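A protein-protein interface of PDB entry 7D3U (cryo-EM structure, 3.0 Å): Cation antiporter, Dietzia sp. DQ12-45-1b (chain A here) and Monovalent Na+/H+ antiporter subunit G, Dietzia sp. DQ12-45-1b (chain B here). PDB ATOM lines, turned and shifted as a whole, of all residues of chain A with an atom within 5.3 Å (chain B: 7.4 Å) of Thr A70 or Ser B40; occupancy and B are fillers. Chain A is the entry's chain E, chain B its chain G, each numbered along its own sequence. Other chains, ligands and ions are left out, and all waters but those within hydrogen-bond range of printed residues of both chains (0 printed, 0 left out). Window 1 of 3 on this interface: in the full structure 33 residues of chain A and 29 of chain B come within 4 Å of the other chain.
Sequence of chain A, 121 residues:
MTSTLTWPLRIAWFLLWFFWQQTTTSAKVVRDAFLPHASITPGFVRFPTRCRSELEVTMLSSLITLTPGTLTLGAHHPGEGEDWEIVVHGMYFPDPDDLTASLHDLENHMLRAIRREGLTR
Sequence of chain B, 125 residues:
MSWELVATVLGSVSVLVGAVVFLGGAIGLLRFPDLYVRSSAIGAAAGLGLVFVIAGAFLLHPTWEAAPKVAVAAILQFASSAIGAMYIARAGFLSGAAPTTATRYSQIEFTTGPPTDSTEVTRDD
Hydrophobic or aromatic side chains of chain A within 4 Å of the printed part of chain B: Leu A71, His A89 and Met A91.
Along chain A the printed residues that touch a printed residue of chain B span positions 70 to 91.
Among the printed residues, 9 pairs touch across the chains.
Among the printed residues, no Asp or Glu carboxylate lies within 4 Å of a Lys or Arg side-chain nitrogen of the other chain.
The side-chain sulfur of Met A91 is in hydrogen-bond range of the side-chain hydroxyl of Ser B40 (2.6 Å).
Among the printed residues, pairs that only touch across the chains: Thr A70 with Ser B40, Leu A71 with Tyr B36, His A89 with Tyr B36, Leu A71 with Ser B40, Leu A71 with Ala B89, His A89 with Val B37, Met A91 with Val B37 and Leu A71 with Ser B39.
N of His A89 is in hydrogen-bond range of O of Leu A71, 2.6 Å away.
O of Ile A64 is in hydrogen-bond range of OG1 of Thr A70, at 2.5 Å.
The side-chain hydroxyl of Ser B40 lies within hydrogen-bond range of the backbone carbonyl oxygen of Tyr B36.
O of Gly A69 is in hydrogen-bond range of N of Met A91 (2.9 Å).
O of Leu B35 lies within hydrogen-bond range of OG of Ser B39, 2.9 Å away.
The backbone carbonyl oxygen of Val B37 sits at hydrogen-bond distance from the side-chain hydroxyl of Ser B40 (2.7 Å).
Thr A70 touches just one residue of chain B: Ser B40.
Of chain A, only Thr A70 (3.5 Å), Leu A71 (3.6 Å) and Met A91 (2.6 Å) come within 4 Å of Ser B40.
No residue of chain B comes within 4 Å of Gly A69.
Of the printed residues of chain A, Ser B39 touches Leu A71 (3.8 Å).
Of the printed residues of chain B, Leu A71 touches Tyr B36, Ser B39, Ser B40 and Ala B89.
Leu A99 touches none of the printed residues of chain B.
Ile A64 touches none of the printed residues of chain B.
The nearest residue of chain B that does not touch Thr A70 is Ala B41 (5.6 Å).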
ATOM      1  N   ILE A  64     -10.433  -5.752  -9.501  1.00  0.00           N
ATOM      2  CA  ILE A  64     -11.203  -4.593  -9.937  1.00  0.00           C
ATOM      3  C   ILE A  64     -11.021  -3.440  -8.959  1.00  0.00           C
ATOM      4  O   ILE A  64     -10.879  -2.280  -9.363  1.00  0.00           O
ATOM      5  CB  ILE A  64     -12.685  -4.968 -10.099  1.00  0.00           C
ATOM      6  CG1 ILE A  64     -12.882  -5.851 -11.329  1.00  0.00           C
ATOM      7  CG2 ILE A  64     -13.540  -3.725 -10.209  1.00  0.00           C
ATOM      8  CD1 ILE A  64     -14.329  -6.017 -11.725  1.00  0.00           C
ATOM      9  N   THR A  65     -11.012  -3.741  -7.660  1.00  0.00           N
ATOM     10  CA  THR A  65     -10.855  -2.692  -6.657  1.00  0.00           C
ATOM     11  C   THR A  65      -9.470  -2.065  -6.728  1.00  0.00           C
ATOM     12  O   THR A  65      -9.332  -0.837  -6.703  1.00  0.00           O
ATOM     13  CB  THR A  65     -11.119  -3.256  -5.263  1.00  0.00           C
ATOM     14  OG1 THR A  65     -12.484  -3.674  -5.171  1.00  0.00           O
ATOM     15  CG2 THR A  65     -10.852  -2.203  -4.205  1.00  0.00           C
ATOM     16  N   THR A  67      -7.604  -1.743  -9.189  1.00  0.00           N
ATOM     17  CA  THR A  67      -7.516  -0.864 -10.344  1.00  0.00           C
ATOM     18  C   THR A  67      -7.889   0.557  -9.925  1.00  0.00           C
ATOM     19  O   THR A  67      -8.877   0.753  -9.210  1.00  0.00           O
ATOM     20  CB  THR A  67      -8.442  -1.354 -11.459  1.00  0.00           C
ATOM     21  OG1 THR A  67      -8.326  -2.775 -11.582  1.00  0.00           O
ATOM     22  CG2 THR A  67      -8.079  -0.713 -12.785  1.00  0.00           C
ATOM     23  N   PRO A  68      -7.122   1.569 -10.341  1.00  0.00           N
ATOM     24  CA  PRO A  68      -7.341   2.927  -9.819  1.00  0.00           C
ATOM     25  C   PRO A  68      -8.612   3.602 -10.308  1.00  0.00           C
ATOM     26  O   PRO A  68      -8.825   4.774  -9.980  1.00  0.00           O
ATOM     27  CB  PRO A  68      -6.104   3.694 -10.313  1.00  0.00           C
ATOM     28  CG  PRO A  68      -5.115   2.651 -10.688  1.00  0.00           C
ATOM     29  CD  PRO A  68      -5.910   1.493 -11.170  1.00  0.00           C
ATOM     30  N   GLY A  69      -9.463   2.925 -11.070  1.00  0.00           N
ATOM     31  CA  GLY A  69     -10.634   3.589 -11.604  1.00  0.00           C
ATOM     32  C   GLY A  69     -11.953   2.906 -11.310  1.00  0.00           C
ATOM     33  O   GLY A  69     -13.006   3.382 -11.741  1.00  0.00           O
ATOM     34  N   THR A  70     -11.918   1.794 -10.580  1.00  0.00           N
ATOM     35  CA  THR A  70     -13.119   1.019 -10.309  1.00  0.00           C
ATOM     36  C   THR A  70     -13.127   0.593  -8.849  1.00  0.00           C
ATOM     37  O   THR A  70     -12.199   0.880  -8.088  1.00  0.00           O
ATOM     38  CB  THR A  70     -13.213  -0.204 -11.228  1.00  0.00           C
ATOM     39  OG1 THR A  70     -11.991  -0.947 -11.163  1.00  0.00           O
ATOM     40  CG2 THR A  70     -13.469   0.218 -12.665  1.00  0.00           C
ATOM     41  N   LEU A  71     -14.196  -0.102  -8.465  1.00  0.00           N
ATOM     42  CA  LEU A  71     -14.375  -0.637  -7.124  1.00  0.00           C
ATOM     43  C   LEU A  71     -15.564  -1.580  -7.145  1.00  0.00           C
ATOM     44  O   LEU A  71     -16.598  -1.258  -7.734  1.00  0.00           O
ATOM     45  CB  LEU A  71     -14.600   0.479  -6.099  1.00  0.00           C
ATOM     46  CG  LEU A  71     -15.355   0.117  -4.821  1.00  0.00           C
ATOM     47  CD1 LEU A  71     -14.499  -0.742  -3.910  1.00  0.00           C
ATOM     48  CD2 LEU A  71     -15.802   1.377  -4.108  1.00  0.00           C
ATOM     49  N   THR A  72     -15.418  -2.734  -6.504  1.00  0.00           N
ATOM     50  CA  THR A  72     -16.470  -3.741  -6.458  1.00  0.00           C
ATOM     51  C   THR A  72     -17.204  -3.640  -5.129  1.00  0.00           C
ATOM     52  O   THR A  72     -16.617  -3.883  -4.072  1.00  0.00           O
ATOM     53  CB  THR A  72     -15.900  -5.145  -6.634  1.00  0.00           C
ATOM     54  OG1 THR A  72     -15.206  -5.228  -7.882  1.00  0.00           O
ATOM     55  CG2 THR A  72     -17.020  -6.164  -6.618  1.00  0.00           C
ATOM     56  N   VAL A  88     -20.088  -3.205  -9.615  1.00  0.00           N
ATOM     57  CA  VAL A  88     -18.854  -2.450  -9.782  1.00  0.00           C
ATOM     58  C   VAL A  88     -19.189  -0.973  -9.893  1.00  0.00           C
ATOM     59  O   VAL A  88     -20.079  -0.584 -10.657  1.00  0.00           O
ATOM     60  CB  VAL A  88     -18.071  -2.928 -11.014  1.00  0.00           C
ATOM     61  CG1 VAL A  88     -16.737  -2.222 -11.093  1.00  0.00           C
ATOM     62  CG2 VAL A  88     -17.874  -4.426 -10.949  1.00  0.00           C
ATOM     63  N   HIS A  89     -18.470  -0.152  -9.136  1.00  0.00           N
ATOM     64  CA  HIS A  89     -18.581   1.297  -9.200  1.00  0.00           C
ATOM     65  C   HIS A  89     -17.361   1.838  -9.928  1.00  0.00           C
ATOM     66  O   HIS A  89     -16.231   1.446  -9.620  1.00  0.00           O
ATOM     67  CB  HIS A  89     -18.680   1.891  -7.795  1.00  0.00           C
ATOM     68  CG  HIS A  89     -18.587   3.382  -7.760  1.00  0.00           C
ATOM     69  ND1 HIS A  89     -17.385   4.051  -7.698  1.00  0.00           N
ATOM     70  CD2 HIS A  89     -19.549   4.334  -7.763  1.00  0.00           C
ATOM     71  CE1 HIS A  89     -17.610   5.352  -7.672  1.00  0.00           C
ATOM     72  NE2 HIS A  89     -18.915   5.550  -7.708  1.00  0.00           N
ATOM     73  N   GLY A  90     -17.581   2.725 -10.881  1.00  0.00           N
ATOM     74  CA  GLY A  90     -16.507   3.199 -11.740  1.00  0.00           C
ATOM     75  C   GLY A  90     -16.455   4.707 -11.838  1.00  0.00           C
ATOM     76  O   GLY A  90     -17.473   5.363 -12.047  1.00  0.00           O
ATOM     77  N   MET A  91     -15.252   5.247 -11.682  1.00  0.00           N
ATOM     78  CA  MET A  91     -15.009   6.668 -11.876  1.00  0.00           C
ATOM     79  C   MET A  91     -14.516   6.928 -13.294  1.00  0.00           C
ATOM     80  O   MET A  91     -13.897   6.066 -13.922  1.00  0.00           O
ATOM     81  CB  MET A  91     -13.985   7.188 -10.869  1.00  0.00           C
ATOM     82  CG  MET A  91     -14.129   6.601  -9.480  1.00  0.00           C
ATOM     83  SD  MET A  91     -12.579   6.636  -8.559  1.00  0.00           S
ATOM     84  CE  MET A  91     -11.881   8.183  -9.127  1.00  0.00           C
ATOM     85  N   PHE A  93     -15.960   6.960 -16.136  1.00  0.00           N
ATOM     86  CA  PHE A  93     -16.474   6.034 -17.143  1.00  0.00           C
ATOM     87  C   PHE A  93     -17.862   6.529 -17.518  1.00  0.00           C
ATOM     88  O   PHE A  93     -18.872   6.039 -16.996  1.00  0.00           O
ATOM     89  CB  PHE A  93     -16.505   4.596 -16.624  1.00  0.00           C
ATOM     90  CG  PHE A  93     -15.177   3.898 -16.691  1.00  0.00           C
ATOM     91  CD1 PHE A  93     -14.562   3.670 -17.908  1.00  0.00           C
ATOM     92  CD2 PHE A  93     -14.550   3.464 -15.536  1.00  0.00           C
ATOM     93  CE1 PHE A  93     -13.342   3.025 -17.972  1.00  0.00           C
ATOM     94  CE2 PHE A  93     -13.330   2.819 -15.594  1.00  0.00           C
ATOM     95  CZ  PHE A  93     -12.726   2.599 -16.814  1.00  0.00           C
ATOM     96  N   LEU A  99     -17.348   0.873 -19.213  1.00  0.00           N
ATOM     97  CA  LEU A  99     -16.994   0.218 -17.960  1.00  0.00           C
ATOM     98  C   LEU A  99     -17.064  -1.297 -18.096  1.00  0.00           C
ATOM     99  O   LEU A  99     -16.146  -2.010 -17.678  1.00  0.00           O
ATOM    100  CB  LEU A  99     -17.917   0.710 -16.844  1.00  0.00           C
ATOM    101  CG  LEU A  99     -17.669   0.169 -15.438  1.00  0.00           C
ATOM    102  CD1 LEU A  99     -16.201   0.279 -15.088  1.00  0.00           C
ATOM    103  CD2 LEU A  99     -18.518   0.914 -14.424  1.00  0.00           C
ATOM    104  N   LEU A 103     -14.057  -4.043 -17.791  1.00  0.00           N
ATOM    105  CA  LEU A 103     -14.167  -5.151 -16.849  1.00  0.00           C
ATOM    106  C   LEU A 103     -14.060  -6.493 -17.557  1.00  0.00           C
ATOM    107  O   LEU A 103     -13.485  -7.439 -17.014  1.00  0.00           O
ATOM    108  CB  LEU A 103     -15.480  -5.061 -16.077  1.00  0.00           C
ATOM    109  CG  LEU A 103     -15.655  -3.815 -15.215  1.00  0.00           C
ATOM    110  CD1 LEU A 103     -16.890  -3.950 -14.355  1.00  0.00           C
ATOM    111  CD2 LEU A 103     -14.420  -3.560 -14.371  1.00  0.00           C
ATOM    112  N   PHE B  32     -12.935  14.609  -3.104  1.00  0.00           N
ATOM    113  CA  PHE B  32     -13.743  13.599  -3.774  1.00  0.00           C
ATOM    114  C   PHE B  32     -15.151  13.667  -3.199  1.00  0.00           C
ATOM    115  O   PHE B  32     -15.320  13.641  -1.968  1.00  0.00           O
ATOM    116  CB  PHE B  32     -13.160  12.190  -3.604  1.00  0.00           C
ATOM    117  CG  PHE B  32     -12.140  11.823  -4.648  1.00  0.00           C
ATOM    118  CD1 PHE B  32     -12.110  12.473  -5.865  1.00  0.00           C
ATOM    119  CD2 PHE B  32     -11.216  10.822  -4.411  1.00  0.00           C
ATOM    120  CE1 PHE B  32     -11.174  12.141  -6.821  1.00  0.00           C
ATOM    121  CE2 PHE B  32     -10.279  10.486  -5.362  1.00  0.00           C
ATOM    122  CZ  PHE B  32     -10.260  11.145  -6.568  1.00  0.00           C
ATOM    123  N   LEU B  35     -18.643   8.727  -1.245  1.00  0.00           N
ATOM    124  CA  LEU B  35     -17.969   7.704  -0.458  1.00  0.00           C
ATOM    125  C   LEU B  35     -17.405   6.612  -1.350  1.00  0.00           C
ATOM    126  O   LEU B  35     -16.378   6.010  -1.019  1.00  0.00           O
ATOM    127  CB  LEU B  35     -18.936   7.098   0.561  1.00  0.00           C
ATOM    128  CG  LEU B  35     -18.431   6.025   1.530  1.00  0.00           C
ATOM    129  CD1 LEU B  35     -19.204   6.118   2.816  1.00  0.00           C
ATOM    130  CD2 LEU B  35     -18.573   4.627   0.958  1.00  0.00           C
ATOM    131  N   TYR B  36     -18.062   6.346  -2.479  1.00  0.00           N
ATOM    132  CA  TYR B  36     -17.638   5.271  -3.362  1.00  0.00           C
ATOM    133  C   TYR B  36     -16.439   5.683  -4.202  1.00  0.00           C
ATOM    134  O   TYR B  36     -15.575   4.854  -4.499  1.00  0.00           O
ATOM    135  CB  TYR B  36     -18.807   4.842  -4.243  1.00  0.00           C
ATOM    136  CG  TYR B  36     -20.085   4.679  -3.458  1.00  0.00           C
ATOM    137  CD1 TYR B  36     -20.310   3.546  -2.693  1.00  0.00           C
ATOM    138  CD2 TYR B  36     -21.054   5.669  -3.463  1.00  0.00           C
ATOM    139  CE1 TYR B  36     -21.467   3.398  -1.967  1.00  0.00           C
ATOM    140  CE2 TYR B  36     -22.215   5.529  -2.740  1.00  0.00           C
ATOM    141  CZ  TYR B  36     -22.416   4.392  -1.993  1.00  0.00           C
ATOM    142  OH  TYR B  36     -23.574   4.249  -1.270  1.00  0.00           O
ATOM    143  N   VAL B  37     -16.367   6.957  -4.592  1.00  0.00           N
ATOM    144  CA  VAL B  37     -15.150   7.463  -5.219  1.00  0.00           C
ATOM    145  C   VAL B  37     -13.993   7.410  -4.232  1.00  0.00           C
ATOM    146  O   VAL B  37     -12.874   7.003  -4.577  1.00  0.00           O
ATOM    147  CB  VAL B  37     -15.376   8.890  -5.751  1.00  0.00           C
ATOM    148  CG1 VAL B  37     -14.111   9.421  -6.388  1.00  0.00           C
ATOM    149  CG2 VAL B  37     -16.519   8.907  -6.744  1.00  0.00           C
ATOM    150  N   ARG B  38     -14.249   7.804  -2.983  1.00  0.00           N
ATOM    151  CA  ARG B  38     -13.214   7.754  -1.957  1.00  0.00           C
ATOM    152  C   ARG B  38     -12.716   6.332  -1.754  1.00  0.00           C
ATOM    153  O   ARG B  38     -11.507   6.092  -1.690  1.00  0.00           O
ATOM    154  CB  ARG B  38     -13.749   8.326  -0.644  1.00  0.00           C
ATOM    155  CG  ARG B  38     -13.617   9.829  -0.526  1.00  0.00           C
ATOM    156  CD  ARG B  38     -14.441  10.360   0.627  1.00  0.00           C
ATOM    157  NE  ARG B  38     -14.664  11.796   0.508  1.00  0.00           N
ATOM    158  CZ  ARG B  38     -15.756  12.418   0.936  1.00  0.00           C
ATOM    159  NH1 ARG B  38     -16.730  11.730   1.512  1.00  0.00           N
ATOM    160  NH2 ARG B  38     -15.874  13.730   0.785  1.00  0.00           N
ATOM    161  N   SER B  39     -13.637   5.373  -1.656  1.00  0.00           N
ATOM    162  CA  SER B  39     -13.231   3.988  -1.441  1.00  0.00           C
ATOM    163  C   SER B  39     -12.525   3.423  -2.665  1.00  0.00           C
ATOM    164  O   SER B  39     -11.575   2.644  -2.532  1.00  0.00           O
ATOM    165  CB  SER B  39     -14.446   3.136  -1.080  1.00  0.00           C
ATOM    166  OG  SER B  39     -15.099   3.647   0.067  1.00  0.00           O
ATOM    167  N   SER B  40     -12.968   3.806  -3.863  1.00  0.00           N
ATOM    168  CA  SER B  40     -12.312   3.335  -5.077  1.00  0.00           C
ATOM    169  C   SER B  40     -10.890   3.863  -5.181  1.00  0.00           C
ATOM    170  O   SER B  40     -10.010   3.173  -5.706  1.00  0.00           O
ATOM    171  CB  SER B  40     -13.121   3.750  -6.305  1.00  0.00           C
ATOM    172  OG  SER B  40     -13.106   5.156  -6.470  1.00  0.00           O
ATOM    173  N   ALA B  41     -10.645   5.078  -4.691  1.00  0.00           N
ATOM    174  CA  ALA B  41      -9.283   5.598  -4.679  1.00  0.00           C
ATOM    175  C   ALA B  41      -8.453   4.967  -3.565  1.00  0.00           C
ATOM    176  O   ALA B  41      -7.267   4.675  -3.760  1.00  0.00           O
ATOM    177  CB  ALA B  41      -9.297   7.119  -4.535  1.00  0.00           C
ATOM    178  N   ILE B  42      -9.064   4.743  -2.400  1.00  0.00           N
ATOM    179  CA  ILE B  42      -8.323   4.222  -1.256  1.00  0.00           C
ATOM    180  C   ILE B  42      -7.906   2.777  -1.495  1.00  0.00           C
ATOM    181  O   ILE B  42      -6.771   2.395  -1.197  1.00  0.00           O
ATOM    182  CB  ILE B  42      -9.154   4.368   0.031  1.00  0.00           C
ATOM    183  CG1 ILE B  42      -9.205   5.830   0.466  1.00  0.00           C
ATOM    184  CG2 ILE B  42      -8.573   3.513   1.141  1.00  0.00           C
ATOM    185  CD1 ILE B  42      -7.862   6.500   0.500  1.00  0.00           C
ATOM    186  N   GLY B  43      -8.809   1.956  -2.038  1.00  0.00           N
ATOM    187  CA  GLY B  43      -8.478   0.565  -2.297  1.00  0.00           C
ATOM    188  C   GLY B  43      -7.210   0.388  -3.104  1.00  0.00           C
ATOM    189  O   GLY B  43      -6.502  -0.609  -2.947  1.00  0.00           O
ATOM    190  N   ALA B  44      -6.899   1.348  -3.972  1.00  0.00           N
ATOM    191  CA  ALA B  44      -5.658   1.308  -4.732  1.00  0.00           C
ATOM    192  C   ALA B  44      -4.515   2.006  -4.007  1.00  0.00           C
ATOM    193  O   ALA B  44      -3.394   1.487  -3.979  1.00  0.00           O
ATOM    194  CB  ALA B  44      -5.863   1.942  -6.109  1.00  0.00           C
ATOM    195  N   ALA B  45      -4.776   3.172  -3.410  1.00  0.00           N
ATOM    196  CA  ALA B  45      -3.698   3.946  -2.803  1.00  0.00           C
ATOM    197  C   ALA B  45      -3.134   3.246  -1.574  1.00  0.00           C
ATOM    198  O   ALA B  45      -1.923   3.014  -1.480  1.00  0.00           O
ATOM    199  CB  ALA B  45      -4.197   5.344  -2.446  1.00  0.00           C
ATOM    200  N   ALA B  85     -11.715  -1.931   1.699  1.00  0.00           N
ATOM    201  CA  ALA B  85     -12.413  -0.892   0.952  1.00  0.00           C
ATOM    202  C   ALA B  85     -13.702  -1.425   0.341  1.00  0.00           C
ATOM    203  O   ALA B  85     -14.724  -0.728   0.330  1.00  0.00           O
ATOM    204  CB  ALA B  85     -11.502  -0.319  -0.131  1.00  0.00           C
ATOM    205  N   ALA B  89     -17.300   0.206   1.370  1.00  0.00           N
ATOM    206  CA  ALA B  89     -18.224   0.753   0.382  1.00  0.00           C
ATOM    207  C   ALA B  89     -19.573   0.049   0.437  1.00  0.00           C
ATOM    208  O   ALA B  89     -20.624   0.698   0.356  1.00  0.00           O
ATOM    209  CB  ALA B  89     -17.620   0.647  -1.016  1.00  0.00           C
